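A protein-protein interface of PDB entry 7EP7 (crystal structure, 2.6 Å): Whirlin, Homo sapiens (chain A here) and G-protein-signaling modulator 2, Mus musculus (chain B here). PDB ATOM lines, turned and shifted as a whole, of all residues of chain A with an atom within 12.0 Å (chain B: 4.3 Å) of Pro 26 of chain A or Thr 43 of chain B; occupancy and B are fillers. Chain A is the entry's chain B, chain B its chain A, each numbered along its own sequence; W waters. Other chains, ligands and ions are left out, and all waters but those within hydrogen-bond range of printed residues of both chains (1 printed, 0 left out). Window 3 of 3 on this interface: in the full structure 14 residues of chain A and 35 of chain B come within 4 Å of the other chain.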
ATOM      1  N   VAL A  22     -16.579 -19.854 -14.419  1.00  0.00           N
ATOM      2  CA  VAL A  22     -15.752 -19.179 -15.399  1.00  0.00           C
ATOM      3  C   VAL A  22     -15.273 -17.880 -14.765  1.00  0.00           C
ATOM      4  O   VAL A  22     -16.001 -17.229 -13.999  1.00  0.00           O
ATOM      5  CB  VAL A  22     -16.506 -18.979 -16.729  1.00  0.00           C
ATOM      6  CG1 VAL A  22     -15.652 -18.216 -17.721  1.00  0.00           C
ATOM      7  CG2 VAL A  22     -16.852 -20.368 -17.301  1.00  0.00           C
ATOM      8  N   ARG A  23     -14.008 -17.549 -15.014  1.00  0.00           N
ATOM      9  CA  ARG A  23     -13.334 -16.437 -14.355  1.00  0.00           C
ATOM     10  C   ARG A  23     -12.743 -15.605 -15.505  1.00  0.00           C
ATOM     11  O   ARG A  23     -11.558 -15.728 -15.841  1.00  0.00           O
ATOM     12  CB  ARG A  23     -12.299 -16.999 -13.347  1.00  0.00           C
ATOM     13  CG  ARG A  23     -11.561 -16.024 -12.447  1.00  0.00           C
ATOM     14  CD  ARG A  23     -10.871 -16.801 -11.322  1.00  0.00           C
ATOM     15  NE  ARG A  23      -9.707 -16.085 -10.800  1.00  0.00           N
ATOM     16  CZ  ARG A  23      -9.772 -15.004 -10.024  1.00  0.00           C
ATOM     17  NH1 ARG A  23     -10.964 -14.506  -9.658  1.00  0.00           N
ATOM     18  NH2 ARG A  23      -8.639 -14.415  -9.623  1.00  0.00           N
ATOM     19  N   ALA A  24     -13.606 -14.785 -16.129  1.00  0.00           N
ATOM     20  CA  ALA A  24     -13.316 -14.088 -17.383  1.00  0.00           C
ATOM     21  C   ALA A  24     -12.130 -13.131 -17.225  1.00  0.00           C
ATOM     22  O   ALA A  24     -11.670 -12.825 -16.115  1.00  0.00           O
ATOM     23  CB  ALA A  24     -14.547 -13.328 -17.885  1.00  0.00           C
ATOM     24  N   LEU A  25     -11.652 -12.631 -18.370  1.00  0.00           N
ATOM     25  CA  LEU A  25     -10.321 -12.036 -18.451  1.00  0.00           C
ATOM     26  C   LEU A  25     -10.414 -10.529 -18.203  1.00  0.00           C
ATOM     27  O   LEU A  25     -11.084  -9.836 -18.979  1.00  0.00           O
ATOM     28  CB  LEU A  25      -9.708 -12.281 -19.816  1.00  0.00           C
ATOM     29  CG  LEU A  25      -9.253 -13.701 -20.166  1.00  0.00           C
ATOM     30  CD1 LEU A  25      -8.308 -14.312 -19.143  1.00  0.00           C
ATOM     31  CD2 LEU A  25     -10.432 -14.581 -20.466  1.00  0.00           C
ATOM     32  N   PRO A  26      -9.751  -9.983 -17.190  1.00  0.00           N
ATOM     33  CA  PRO A  26     -10.032  -8.601 -16.775  1.00  0.00           C
ATOM     34  C   PRO A  26      -9.200  -7.547 -17.493  1.00  0.00           C
ATOM     35  O   PRO A  26      -8.009  -7.728 -17.764  1.00  0.00           O
ATOM     36  CB  PRO A  26      -9.698  -8.624 -15.274  1.00  0.00           C
ATOM     37  CG  PRO A  26      -8.850  -9.921 -15.040  1.00  0.00           C
ATOM     38  CD  PRO A  26      -8.669 -10.577 -16.385  1.00  0.00           C
ATOM     39  N   GLN A  27      -9.858  -6.428 -17.805  1.00  0.00           N
ATOM     40  CA  GLN A  27      -9.184  -5.182 -18.202  1.00  0.00           C
ATOM     41  C   GLN A  27      -9.432  -4.081 -17.167  1.00  0.00           C
ATOM     42  O   GLN A  27      -8.966  -4.166 -16.022  1.00  0.00           O
ATOM     43  CB  GLN A  27      -9.648  -4.704 -19.584  1.00  0.00           C
ATOM     44  CG  GLN A  27      -8.967  -5.413 -20.740  1.00  0.00           C
ATOM     45  CD  GLN A  27      -9.800  -6.548 -21.303  1.00  0.00           C
ATOM     46  OE1 GLN A  27     -10.354  -7.359 -20.551  1.00  0.00           O
ATOM     47  NE2 GLN A  27      -9.881  -6.622 -22.635  1.00  0.00           N
ATOM     48  N   LEU B   8      -2.691 -10.789 -22.598  1.00  0.00           N
ATOM     49  CA  LEU B   8      -4.136 -10.702 -22.440  1.00  0.00           C
ATOM     50  C   LEU B   8      -4.810 -10.872 -23.801  1.00  0.00           C
ATOM     51  O   LEU B   8      -5.832 -11.563 -23.940  1.00  0.00           O
ATOM     52  CB  LEU B   8      -4.475  -9.358 -21.788  1.00  0.00           C
ATOM     53  CG  LEU B   8      -5.796  -9.129 -21.040  1.00  0.00           C
ATOM     54  CD1 LEU B   8      -5.644  -7.943 -20.058  1.00  0.00           C
ATOM     55  CD2 LEU B   8      -6.988  -8.994 -21.906  1.00  0.00           C
ATOM     56  N   ASP B  40       0.182  -9.100 -14.010  1.00  0.00           N
ATOM     57  CA  ASP B  40      -1.029  -8.958 -13.217  1.00  0.00           C
ATOM     58  C   ASP B  40      -1.460 -10.353 -12.794  1.00  0.00           C
ATOM     59  O   ASP B  40      -1.825 -11.181 -13.638  1.00  0.00           O
ATOM     60  CB  ASP B  40      -2.149  -8.248 -13.976  1.00  0.00           C
ATOM     61  CG  ASP B  40      -3.382  -8.060 -13.117  1.00  0.00           C
ATOM     62  OD1 ASP B  40      -4.422  -7.590 -13.628  1.00  0.00           O
ATOM     63  OD2 ASP B  40      -3.319  -8.400 -11.915  1.00  0.00           O
ATOM     64  N   LEU B  41      -1.405 -10.609 -11.487  1.00  0.00           N
ATOM     65  CA  LEU B  41      -1.597 -11.970 -11.014  1.00  0.00           C
ATOM     66  C   LEU B  41      -3.052 -12.404 -11.116  1.00  0.00           C
ATOM     67  O   LEU B  41      -3.305 -13.583 -11.387  1.00  0.00           O
ATOM     68  CB  LEU B  41      -1.073 -12.119  -9.589  1.00  0.00           C
ATOM     69  CG  LEU B  41       0.436 -12.363  -9.481  1.00  0.00           C
ATOM     70  CD1 LEU B  41       0.816 -12.583  -8.026  1.00  0.00           C
ATOM     71  CD2 LEU B  41       0.936 -13.534 -10.357  1.00  0.00           C
ATOM     72  N   LYS B  42      -4.018 -11.492 -10.927  1.00  0.00           N
ATOM     73  CA  LYS B  42      -5.394 -11.872 -11.220  1.00  0.00           C
ATOM     74  C   LYS B  42      -5.588 -12.221 -12.681  1.00  0.00           C
ATOM     75  O   LYS B  42      -6.489 -13.002 -12.999  1.00  0.00           O
ATOM     76  CB  LYS B  42      -6.409 -10.791 -10.842  1.00  0.00           C
ATOM     77  CG  LYS B  42      -6.920 -10.943  -9.428  1.00  0.00           C
ATOM     78  CD  LYS B  42      -7.736  -9.750  -8.930  1.00  0.00           C
ATOM     79  CE  LYS B  42      -9.203  -9.844  -9.370  1.00  0.00           C
ATOM     80  NZ  LYS B  42     -10.162  -9.374  -8.321  1.00  0.00           N
ATOM     81  N   THR B  43      -4.773 -11.678 -13.577  1.00  0.00           N
ATOM     82  CA  THR B  43      -4.994 -12.000 -14.981  1.00  0.00           C
ATOM     83  C   THR B  43      -4.454 -13.392 -15.301  1.00  0.00           C
ATOM     84  O   THR B  43      -5.148 -14.209 -15.927  1.00  0.00           O
ATOM     85  CB  THR B  43      -4.361 -10.926 -15.876  1.00  0.00           C
ATOM     86  OG1 THR B  43      -4.936  -9.650 -15.549  1.00  0.00           O
ATOM     87  CG2 THR B  43      -4.655 -11.212 -17.338  1.00  0.00           C
ATOM     88  N   LEU B  44      -3.221 -13.672 -14.846  1.00  0.00           N
ATOM     89  CA  LEU B  44      -2.615 -14.994 -14.989  1.00  0.00           C
ATOM     90  C   LEU B  44      -3.456 -16.067 -14.315  1.00  0.00           C
ATOM     91  O   LEU B  44      -3.672 -17.152 -14.876  1.00  0.00           O
ATOM     92  CB  LEU B  44      -1.216 -14.983 -14.378  1.00  0.00           C
ATOM     93  CG  LEU B  44      -0.151 -15.969 -14.865  1.00  0.00           C
ATOM     94  CD1 LEU B  44       0.041 -15.879 -16.352  1.00  0.00           C
ATOM     95  CD2 LEU B  44       1.114 -15.635 -14.145  1.00  0.00           C
ATOM     96  N   SER B  45      -3.946 -15.782 -13.112  1.00  0.00           N
ATOM     97  CA  SER B  45      -4.786 -16.744 -12.415  1.00  0.00           C
ATOM     98  C   SER B  45      -6.049 -17.044 -13.234  1.00  0.00           C
ATOM     99  O   SER B  45      -6.435 -18.213 -13.401  1.00  0.00           O
ATOM    100  CB  SER B  45      -5.101 -16.192 -11.010  1.00  0.00           C
ATOM    101  OG  SER B  45      -5.823 -17.084 -10.180  1.00  0.00           O
ATOM    102  N   ALA B  46      -6.664 -16.004 -13.802  1.00  0.00           N
ATOM    103  CA  ALA B  46      -7.839 -16.192 -14.646  1.00  0.00           C
ATOM    104  C   ALA B  46      -7.527 -17.042 -15.871  1.00  0.00           C
ATOM    105  O   ALA B  46      -8.387 -17.797 -16.347  1.00  0.00           O
ATOM    106  CB  ALA B  46      -8.389 -14.842 -15.066  1.00  0.00           C
ATOM    107  N   ILE B  47      -6.301 -16.942 -16.388  1.00  0.00           N
ATOM    108  CA  ILE B  47      -5.879 -17.790 -17.504  1.00  0.00           C
ATOM    109  C   ILE B  47      -5.734 -19.242 -17.049  1.00  0.00           C
ATOM    110  O   ILE B  47      -6.144 -20.179 -17.750  1.00  0.00           O
ATOM    111  CB  ILE B  47      -4.565 -17.253 -18.104  1.00  0.00           C
ATOM    112  CG1 ILE B  47      -4.794 -15.907 -18.780  1.00  0.00           C
ATOM    113  CG2 ILE B  47      -3.925 -18.255 -19.051  1.00  0.00           C
ATOM    114  CD1 ILE B  47      -3.544 -15.053 -18.836  1.00  0.00           C
HETATM  115  O   HOH W   1      -7.781 -16.351  -8.025  1.00  0.00           O
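The backbone NH (N) of Lys 42 of chain B sits at hydrogen-bond distance from the side-chain carboxylate (OD2) of Asp 40 of chain B.
The side-chain carboxylate of Asp 40 of chain B is in hydrogen-bond range of the side-chain hydroxyl of Thr 43 of chain B (2.9 Å).
The backbone carbonyl oxygen (O) of Leu 25 of chain A lies close to the side-chain amide oxygen (OE1) of Gln 27 of chain A (3.0 Å).
Among the printed residues, merely in contact across the chains: Arg 23 of chain A with Lys 42 of chain B (3.9 Å), Arg 23 of chain A with Ser 45 of chain B (3.9 Å), Arg 23 of chain A with Ala 46 of chain B (3.4 Å), Ala 24 of chain A with Ala 46 of chain B (3.99 Å), Leu 25 of chain A with Ile 47 of chain B (3.9 Å), Pro 26 of chain A with Leu 8 of chain B (3.3 Å), Pro 26 of chain A with Thr 43 of chain B (3.9 Å) and Gln 27 of chain A with Leu 8 of chain B (3.8 Å).
Val 22 of chain A touches none of the printed residues of chain B.
Of the printed residues of chain B, Arg 23 of chain A touches Lys 42, Ser 45 and Ala 46.
Printed residues of chain B within 4 Å of Leu 25 of chain A: Ile 47 (3.9 Å).
Pro 26 of chain A touches two residues of chain B.
Printed residues of chain B within 4 Å of Gln 27 of chain A: Leu 8.
No residue of chain A comes within 4 Å of Asp 40 of chain B.
Leu 41 of chain B touches none of the printed residues of chain A.
Of chain A, only Arg 23 comes within 4 Å of Lys 42 of chain B.
Of chain A, only Pro 26 comes within 4 Å of Thr 43 of chain B.
Leu 44 of chain B touches none of the printed residues of chain A.
Of chain A, only Arg 23 comes within 4 Å of Ser 45 of chain B.
Of chain A, only Leu 25 comes within 4 Å of Ile 47 of chain B.
The nearest residue of chain A that does not touch Thr 43 of chain B is Leu 25 of chain A (4.5 Å).
Of the 9 printed residues of chain B, 6 touch a printed residue of chain A.
Printed residues of chain B that touch a printed residue of chain A: Leu 8, Lys 42, Thr 43, Ser 45, Ala 46 and Ile 47.
Hydrophobic or aromatic side chains of chain B within 4 Å of the printed part of chain A: Leu 8, Ala 46 and Ile 47.
Of the 6 printed residues of chain A, 5 touch a printed residue of chain B.
Printed residues of chain A that touch a printed residue of chain B: Arg 23, Ala 24, Leu 25, Pro 26 and Gln 27.
Among the printed residues, no Asp or Glu carboxylate lies within 4 Å of a Lys or Arg side-chain nitrogen of the other chain.
Water W1 bridges the guanidinium group (NH2) of Arg 23 of chain A (2.7 Å) and the side-chain hydroxyl (OG) of Ser 45 of chain B (3.0 Å).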
